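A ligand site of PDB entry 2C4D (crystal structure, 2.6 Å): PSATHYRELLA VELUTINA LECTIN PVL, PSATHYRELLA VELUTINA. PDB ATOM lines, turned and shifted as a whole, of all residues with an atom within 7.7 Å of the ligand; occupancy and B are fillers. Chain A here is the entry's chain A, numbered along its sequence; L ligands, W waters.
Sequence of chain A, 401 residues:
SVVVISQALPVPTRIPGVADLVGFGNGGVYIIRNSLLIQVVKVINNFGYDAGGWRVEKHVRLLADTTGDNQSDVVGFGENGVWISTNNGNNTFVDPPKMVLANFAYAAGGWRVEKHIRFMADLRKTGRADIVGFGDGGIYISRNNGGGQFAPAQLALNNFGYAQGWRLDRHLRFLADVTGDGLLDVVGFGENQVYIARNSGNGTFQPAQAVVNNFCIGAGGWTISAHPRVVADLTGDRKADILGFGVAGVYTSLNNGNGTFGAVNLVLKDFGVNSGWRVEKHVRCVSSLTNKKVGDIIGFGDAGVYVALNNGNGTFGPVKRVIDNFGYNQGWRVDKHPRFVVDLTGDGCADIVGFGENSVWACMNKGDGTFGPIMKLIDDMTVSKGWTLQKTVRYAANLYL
O2 of the ligand sits at hydrogen-bond distance from OD1 of Asn 46.
The backbone carbonyl oxygen (O) of Gly 52 sits at hydrogen-bond distance from a nitrogen (N1) of the ligand, at 2.7 Å.
An oxygen (O2) of the ligand sits at hydrogen-bond distance from the indole nitrogen of Trp 54 (3.0 Å).
The backbone NH of Glu 79 is in hydrogen-bond range of an oxygen (O6) of the ligand, 3.0 Å away.
NE1 of Trp 54 is in hydrogen-bond range of OD1 of Asn 46 (3.5 Å).
The backbone carbonyl oxygen of Ala 51 lies close to the side-chain amide oxygen of Asn 46.
N of Trp 54 sits at hydrogen-bond distance from O of Gly 48 (3.0 Å).
OE1 of Glu 79 lies within hydrogen-bond range of NE2 of His 59, at 2.7 Å.
The side-chain carboxylate (OE2) of Glu 79 is in salt-bridge range of the side-chain amino group (NZ) of Lys 58, at 2.4 Å.
A ring nitrogen (ND1) of His 59 is in hydrogen-bond range of the backbone NH (N) of Arg 55, 3.0 Å away.
N of Gly 76 sits at hydrogen-bond distance from O of Trp 83, 2.8 Å away.
O of Gly 48 sits at hydrogen-bond distance from N of Gly 53 (3.5 Å).
Gly 53 touches the ligand.
His 59 touches the ligand (NE2 to C8, 3.4 Å).
CA of Gly 78 touches O6 of the ligand (3.5 Å).
CH2 of Trp 83 touches C6 of the ligand, 3.7 Å away.
Hydrophobic or aromatic side chains that line the ligand: Trp 54, His 59 and Trp 83.
Within 4 Å of the ligand: Asn 46, Gly 52, Gly 53, Trp 54, His 59, Gly 78, Glu 79 and Trp 83.
The nearest printed residue that does not touch the ligand is Asn 80 (4.1 Å).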
ATOM      1  N   ASN A  45      27.260  20.541 -29.061  1.00  0.00           N
ATOM      2  CA  ASN A  45      26.843  19.294 -29.679  1.00  0.00           C
ATOM      3  C   ASN A  45      27.210  18.096 -28.753  1.00  0.00           C
ATOM      4  O   ASN A  45      28.095  17.280 -29.010  1.00  0.00           O
ATOM      5  CB  ASN A  45      27.339  19.160 -31.126  1.00  0.00           C
ATOM      6  CG  ASN A  45      26.553  18.062 -31.891  1.00  0.00           C
ATOM      7  OD1 ASN A  45      27.125  17.258 -32.618  1.00  0.00           O
ATOM      8  ND2 ASN A  45      25.230  17.994 -31.666  1.00  0.00           N
ATOM      9  N   ASN A  46      26.500  18.044 -27.646  1.00  0.00           N
ATOM     10  CA  ASN A  46      26.777  17.103 -26.590  1.00  0.00           C
ATOM     11  C   ASN A  46      25.744  17.285 -25.476  1.00  0.00           C
ATOM     12  O   ASN A  46      24.881  18.177 -25.546  1.00  0.00           O
ATOM     13  CB  ASN A  46      28.196  17.275 -26.034  1.00  0.00           C
ATOM     14  CG  ASN A  46      28.891  15.926 -25.781  1.00  0.00           C
ATOM     15  OD1 ASN A  46      28.265  14.960 -25.285  1.00  0.00           O
ATOM     16  ND2 ASN A  46      30.181  15.868 -26.102  1.00  0.00           N
ATOM     17  N   PHE A  47      25.816  16.405 -24.475  1.00  0.00           N
ATOM     18  CA  PHE A  47      24.897  16.397 -23.365  1.00  0.00           C
ATOM     19  C   PHE A  47      23.506  16.062 -23.799  1.00  0.00           C
ATOM     20  O   PHE A  47      22.557  16.376 -23.085  1.00  0.00           O
ATOM     21  CB  PHE A  47      24.950  17.713 -22.630  1.00  0.00           C
ATOM     22  CG  PHE A  47      26.299  17.994 -22.026  1.00  0.00           C
ATOM     23  CD1 PHE A  47      26.705  17.337 -20.850  1.00  0.00           C
ATOM     24  CD2 PHE A  47      27.173  18.869 -22.644  1.00  0.00           C
ATOM     25  CE1 PHE A  47      27.933  17.566 -20.285  1.00  0.00           C
ATOM     26  CE2 PHE A  47      28.424  19.115 -22.065  1.00  0.00           C
ATOM     27  CZ  PHE A  47      28.790  18.466 -20.861  1.00  0.00           C
ATOM     28  N   GLY A  48      23.376  15.381 -24.942  1.00  0.00           N
ATOM     29  CA  GLY A  48      22.079  15.101 -25.548  1.00  0.00           C
ATOM     30  C   GLY A  48      21.749  13.638 -25.667  1.00  0.00           C
ATOM     31  O   GLY A  48      22.636  12.812 -25.790  1.00  0.00           O
ATOM     32  N   ALA A  51      23.144  13.204 -28.825  1.00  0.00           N
ATOM     33  CA  ALA A  51      24.484  13.808 -28.794  1.00  0.00           C
ATOM     34  C   ALA A  51      25.354  13.357 -27.572  1.00  0.00           C
ATOM     35  O   ALA A  51      25.623  14.126 -26.631  1.00  0.00           O
ATOM     36  CB  ALA A  51      24.366  15.324 -28.824  1.00  0.00           C
ATOM     37  N   GLY A  52      25.817  12.121 -27.602  1.00  0.00           N
ATOM     38  CA  GLY A  52      26.584  11.592 -26.477  1.00  0.00           C
ATOM     39  C   GLY A  52      25.854  10.528 -25.687  1.00  0.00           C
ATOM     40  O   GLY A  52      26.311  10.131 -24.631  1.00  0.00           O
ATOM     41  N   GLY A  53      24.725  10.074 -26.164  1.00  0.00           N
ATOM     42  CA  GLY A  53      23.953   9.065 -25.431  1.00  0.00           C
ATOM     43  C   GLY A  53      23.458   9.435 -24.018  1.00  0.00           C
ATOM     44  O   GLY A  53      23.326   8.540 -23.169  1.00  0.00           O
ATOM     45  N   TRP A  54      23.124  10.709 -23.743  1.00  0.00           N
ATOM     46  CA  TRP A  54      22.709  11.064 -22.372  1.00  0.00           C
ATOM     47  C   TRP A  54      21.315  10.573 -22.038  1.00  0.00           C
ATOM     48  O   TRP A  54      20.395  10.643 -22.861  1.00  0.00           O
ATOM     49  CB  TRP A  54      22.874  12.556 -22.088  1.00  0.00           C
ATOM     50  CG  TRP A  54      24.310  12.920 -22.102  1.00  0.00           C
ATOM     51  CD1 TRP A  54      25.125  12.963 -23.189  1.00  0.00           C
ATOM     52  CD2 TRP A  54      25.123  13.234 -20.967  1.00  0.00           C
ATOM     53  NE1 TRP A  54      26.400  13.311 -22.826  1.00  0.00           N
ATOM     54  CE2 TRP A  54      26.439  13.479 -21.458  1.00  0.00           C
ATOM     55  CE3 TRP A  54      24.893  13.303 -19.586  1.00  0.00           C
ATOM     56  CZ2 TRP A  54      27.507  13.829 -20.617  1.00  0.00           C
ATOM     57  CZ3 TRP A  54      25.972  13.674 -18.753  1.00  0.00           C
ATOM     58  CH2 TRP A  54      27.253  13.918 -19.272  1.00  0.00           C
ATOM     59  N   ARG A  55      21.169  10.068 -20.816  1.00  0.00           N
ATOM     60  CA  ARG A  55      19.948   9.395 -20.367  1.00  0.00           C
ATOM     61  C   ARG A  55      19.489   9.917 -19.007  1.00  0.00           C
ATOM     62  O   ARG A  55      20.198   9.830 -18.010  1.00  0.00           O
ATOM     63  CB  ARG A  55      20.205   7.883 -20.268  1.00  0.00           C
ATOM     64  CG  ARG A  55      20.397   7.165 -21.599  1.00  0.00           C
ATOM     65  CD  ARG A  55      19.110   7.151 -22.366  1.00  0.00           C
ATOM     66  NE  ARG A  55      19.224   6.562 -23.685  1.00  0.00           N
ATOM     67  CZ  ARG A  55      19.873   7.117 -24.710  1.00  0.00           C
ATOM     68  NH1 ARG A  55      20.556   8.269 -24.617  1.00  0.00           N
ATOM     69  NH2 ARG A  55      19.881   6.477 -25.864  1.00  0.00           N
ATOM     70  N   LYS A  58      20.087   7.605 -16.066  1.00  0.00           N
ATOM     71  CA  LYS A  58      21.468   7.161 -15.814  1.00  0.00           C
ATOM     72  C   LYS A  58      22.443   8.307 -15.513  1.00  0.00           C
ATOM     73  O   LYS A  58      23.479   8.058 -14.921  1.00  0.00           O
ATOM     74  CB  LYS A  58      22.048   6.445 -17.038  1.00  0.00           C
ATOM     75  CG  LYS A  58      21.417   5.092 -17.424  1.00  0.00           C
ATOM     76  CD  LYS A  58      22.170   4.466 -18.603  1.00  0.00           C
ATOM     77  CE  LYS A  58      23.337   3.656 -18.086  1.00  0.00           C
ATOM     78  NZ  LYS A  58      24.582   3.783 -18.877  1.00  0.00           N
ATOM     79  N   HIS A  59      22.123   9.532 -15.973  1.00  0.00           N
ATOM     80  CA  HIS A  59      23.018  10.690 -15.960  1.00  0.00           C
ATOM     81  C   HIS A  59      22.335  11.945 -15.454  1.00  0.00           C
ATOM     82  O   HIS A  59      21.126  12.033 -15.510  1.00  0.00           O
ATOM     83  CB  HIS A  59      23.546  10.965 -17.374  1.00  0.00           C
ATOM     84  CG  HIS A  59      24.092   9.757 -18.056  1.00  0.00           C
ATOM     85  ND1 HIS A  59      23.471   9.163 -19.117  1.00  0.00           N
ATOM     86  CD2 HIS A  59      25.185   9.013 -17.794  1.00  0.00           C
ATOM     87  CE1 HIS A  59      24.140   8.087 -19.479  1.00  0.00           C
ATOM     88  NE2 HIS A  59      25.193   7.978 -18.685  1.00  0.00           N
ATOM     89  N   ARG A  61      22.345  16.213 -15.630  1.00  0.00           N
ATOM     90  CA  ARG A  61      22.784  17.450 -16.271  1.00  0.00           C
ATOM     91  C   ARG A  61      22.342  18.723 -15.513  1.00  0.00           C
ATOM     92  O   ARG A  61      21.146  18.925 -15.232  1.00  0.00           O
ATOM     93  CB  ARG A  61      22.272  17.455 -17.714  1.00  0.00           C
ATOM     94  CG  ARG A  61      23.148  16.624 -18.621  1.00  0.00           C
ATOM     95  CD  ARG A  61      22.476  16.103 -19.859  1.00  0.00           C
ATOM     96  NE  ARG A  61      21.331  15.273 -19.535  1.00  0.00           N
ATOM     97  CZ  ARG A  61      20.438  14.840 -20.426  1.00  0.00           C
ATOM     98  NH1 ARG A  61      20.622  15.099 -21.715  1.00  0.00           N
ATOM     99  NH2 ARG A  61      19.395  14.112 -20.049  1.00  0.00           N
ATOM    100  N   GLY A  76      27.866  17.805 -16.597  1.00  0.00           N
ATOM    101  CA  GLY A  76      27.143  16.548 -16.822  1.00  0.00           C
ATOM    102  C   GLY A  76      27.801  15.401 -16.071  1.00  0.00           C
ATOM    103  O   GLY A  76      29.033  15.216 -16.177  1.00  0.00           O
ATOM    104  N   PHE A  77      27.001  14.657 -15.309  1.00  0.00           N
ATOM    105  CA  PHE A  77      27.485  13.494 -14.590  1.00  0.00           C
ATOM    106  C   PHE A  77      27.195  12.338 -15.488  1.00  0.00           C
ATOM    107  O   PHE A  77      26.068  11.828 -15.511  1.00  0.00           O
ATOM    108  CB  PHE A  77      26.810  13.333 -13.226  1.00  0.00           C
ATOM    109  CG  PHE A  77      27.201  14.391 -12.236  1.00  0.00           C
ATOM    110  CD1 PHE A  77      28.302  14.231 -11.420  1.00  0.00           C
ATOM    111  CD2 PHE A  77      26.469  15.555 -12.123  1.00  0.00           C
ATOM    112  CE1 PHE A  77      28.682  15.205 -10.513  1.00  0.00           C
ATOM    113  CE2 PHE A  77      26.843  16.525 -11.222  1.00  0.00           C
ATOM    114  CZ  PHE A  77      27.967  16.344 -10.428  1.00  0.00           C
ATOM    115  N   GLY A  78      28.202  11.978 -16.280  1.00  0.00           N
ATOM    116  CA  GLY A  78      28.014  11.057 -17.382  1.00  0.00           C
ATOM    117  C   GLY A  78      28.141   9.601 -17.007  1.00  0.00           C
ATOM    118  O   GLY A  78      27.941   9.205 -15.835  1.00  0.00           O
ATOM    119  N   GLU A  79      28.466   8.810 -18.027  1.00  0.00           N
ATOM    120  CA  GLU A  79      28.716   7.380 -17.915  1.00  0.00           C
ATOM    121  C   GLU A  79      30.044   7.013 -17.233  1.00  0.00           C
ATOM    122  O   GLU A  79      30.109   6.063 -16.471  1.00  0.00           O
ATOM    123  CB  GLU A  79      28.742   6.775 -19.324  1.00  0.00           C
ATOM    124  CG  GLU A  79      28.622   5.256 -19.382  1.00  0.00           C
ATOM    125  CD  GLU A  79      27.238   4.772 -19.119  1.00  0.00           C
ATOM    126  OE1 GLU A  79      26.396   5.572 -18.700  1.00  0.00           O
ATOM    127  OE2 GLU A  79      26.959   3.582 -19.323  1.00  0.00           O
ATOM    128  N   ASN A  80      31.093   7.734 -17.581  1.00  0.00           N
ATOM    129  CA  ASN A  80      32.435   7.425 -17.105  1.00  0.00           C
ATOM    130  C   ASN A  80      33.086   8.586 -16.326  1.00  0.00           C
ATOM    131  O   ASN A  80      34.239   8.484 -15.880  1.00  0.00           O
ATOM    132  CB  ASN A  80      33.344   7.014 -18.277  1.00  0.00           C
ATOM    133  CG  ASN A  80      32.755   5.874 -19.107  1.00  0.00           C
ATOM    134  OD1 ASN A  80      32.397   4.808 -18.570  1.00  0.00           O
ATOM    135  ND2 ASN A  80      32.650   6.093 -20.419  1.00  0.00           N
ATOM    136  N   GLY A  81      32.397   9.682 -16.148  1.00  0.00           N
ATOM    137  CA  GLY A  81      33.055  10.760 -15.452  1.00  0.00           C
ATOM    138  C   GLY A  81      32.215  12.004 -15.474  1.00  0.00           C
ATOM    139  O   GLY A  81      31.050  11.922 -15.894  1.00  0.00           O
ATOM    140  N   VAL A  82      32.828  13.120 -15.054  1.00  0.00           N
ATOM    141  CA  VAL A  82      32.156  14.402 -15.008  1.00  0.00           C
ATOM    142  C   VAL A  82      32.688  15.317 -16.103  1.00  0.00           C
ATOM    143  O   VAL A  82      33.888  15.618 -16.154  1.00  0.00           O
ATOM    144  CB  VAL A  82      32.244  15.066 -13.615  1.00  0.00           C
ATOM    145  CG1 VAL A  82      31.706  16.509 -13.639  1.00  0.00           C
ATOM    146  CG2 VAL A  82      31.466  14.242 -12.618  1.00  0.00           C
ATOM    147  N   TRP A  83      31.760  15.779 -16.934  1.00  0.00           N
ATOM    148  CA  TRP A  83      32.052  16.466 -18.162  1.00  0.00           C
ATOM    149  C   TRP A  83      31.557  17.867 -18.051  1.00  0.00           C
ATOM    150  O   TRP A  83      30.389  18.089 -17.820  1.00  0.00           O
ATOM    151  CB  TRP A  83      31.332  15.785 -19.319  1.00  0.00           C
ATOM    152  CG  TRP A  83      31.868  14.449 -19.694  1.00  0.00           C
ATOM    153  CD1 TRP A  83      31.419  13.227 -19.273  1.00  0.00           C
ATOM    154  CD2 TRP A  83      32.923  14.173 -20.623  1.00  0.00           C
ATOM    155  NE1 TRP A  83      32.147  12.217 -19.870  1.00  0.00           N
ATOM    156  CE2 TRP A  83      33.071  12.778 -20.708  1.00  0.00           C
ATOM    157  CE3 TRP A  83      33.779  14.996 -21.395  1.00  0.00           C
ATOM    158  CZ2 TRP A  83      34.002  12.163 -21.522  1.00  0.00           C
ATOM    159  CZ3 TRP A  83      34.720  14.402 -22.202  1.00  0.00           C
ATOM    160  CH2 TRP A  83      34.846  12.990 -22.259  1.00  0.00           C
ATOM    161  N   ASP A  95      33.458  23.404 -26.584  1.00  0.00           N
ATOM    162  CA  ASP A  95      32.856  22.195 -27.173  1.00  0.00           C
ATOM    163  C   ASP A  95      33.935  21.429 -27.943  1.00  0.00           C
ATOM    164  O   ASP A  95      34.505  21.977 -28.854  1.00  0.00           O
ATOM    165  CB  ASP A  95      31.726  22.543 -28.140  1.00  0.00           C
ATOM    166  CG  ASP A  95      30.925  21.325 -28.584  1.00  0.00           C
ATOM    167  OD1 ASP A  95      31.294  20.173 -28.183  1.00  0.00           O
ATOM    168  OD2 ASP A  95      29.905  21.546 -29.303  1.00  0.00           O
ATOM    169  N   PRO A  96      34.220  20.164 -27.573  1.00  0.00           N
ATOM    170  CA  PRO A  96      33.541  19.263 -26.639  1.00  0.00           C
ATOM    171  C   PRO A  96      33.901  19.607 -25.215  1.00  0.00           C
ATOM    172  O   PRO A  96      34.871  20.362 -24.983  1.00  0.00           O
ATOM    173  CB  PRO A  96      34.119  17.883 -26.993  1.00  0.00           C
ATOM    174  CG  PRO A  96      35.516  18.164 -27.400  1.00  0.00           C
ATOM    175  CD  PRO A  96      35.478  19.559 -28.073  1.00  0.00           C
ATOM    176  N   PRO A  97      33.135  19.051 -24.266  1.00  0.00           N
ATOM    177  CA  PRO A  97      33.370  19.302 -22.839  1.00  0.00           C
ATOM    178  C   PRO A  97      34.623  18.518 -22.352  1.00  0.00           C
ATOM    179  O   PRO A  97      35.026  17.552 -23.023  1.00  0.00           O
ATOM    180  CB  PRO A  97      32.109  18.751 -22.187  1.00  0.00           C
ATOM    181  CG  PRO A  97      31.620  17.659 -23.147  1.00  0.00           C
ATOM    182  CD  PRO A  97      32.013  18.109 -24.485  1.00  0.00           C
ATOM    183  N   MET A  99      36.366  16.005 -19.607  1.00  0.00           N
ATOM    184  CA  MET A  99      36.221  15.078 -18.510  1.00  0.00           C
ATOM    185  C   MET A  99      37.175  15.545 -17.401  1.00  0.00           C
ATOM    186  O   MET A  99      38.408  15.558 -17.589  1.00  0.00           O
ATOM    187  CB  MET A  99      36.561  13.670 -18.980  1.00  0.00           C
ATOM    188  CG  MET A  99      35.849  12.556 -18.217  1.00  0.00           C
ATOM    189  SD  MET A  99      36.447  12.470 -16.505  1.00  0.00           S
ATOM    190  CE  MET A  99      38.085  11.811 -16.783  1.00  0.00           C
ATOM    191  N   ALA A 105      29.873   8.917 -11.230  1.00  0.00           N
ATOM    192  CA  ALA A 105      29.383   8.540 -12.524  1.00  0.00           C
ATOM    193  C   ALA A 105      28.944   7.085 -12.543  1.00  0.00           C
ATOM    194  O   ALA A 105      29.353   6.277 -11.740  1.00  0.00           O
ATOM    195  CB  ALA A 105      30.466   8.782 -13.570  1.00  0.00           C
HETATM  196  C1  LIG L   1      30.372   9.546 -23.742  1.00  0.00           C
HETATM  197  C2  LIG L   1      29.662  10.781 -23.200  1.00  0.00           C
HETATM  198  C3  LIG L   1      29.746  11.925 -24.208  1.00  0.00           C
HETATM  199  C4  LIG L   1      31.208  12.155 -24.609  1.00  0.00           C
HETATM  200  C5  LIG L   1      31.939  10.851 -24.980  1.00  0.00           C
HETATM  201  C6  LIG L   1      33.434  11.108 -25.092  1.00  0.00           C
HETATM  202  C7  LIG L   1      27.989  10.173 -21.543  1.00  0.00           C
HETATM  203  C8  LIG L   1      26.569   9.762 -21.239  1.00  0.00           C
HETATM  204  N1  LIG L   1      28.275  10.519 -22.828  1.00  0.00           N
HETATM  205  O1  LIG L   1      30.326   8.491 -22.821  1.00  0.00           O
HETATM  206  O2  LIG L   1      29.233  13.131 -23.654  1.00  0.00           O
HETATM  207  O3  LIG L   1      31.249  13.094 -25.669  1.00  0.00           O
HETATM  208  O4  LIG L   1      31.731   9.863 -23.994  1.00  0.00           O
HETATM  209  O5  LIG L   1      34.042  10.021 -25.728  1.00  0.00           O
HETATM  210  O6  LIG L   1      28.834  10.160 -20.636  1.00  0.00           O
HETATM  211  O   HOH W   1      31.223   9.397 -19.825  1.00  0.00           O
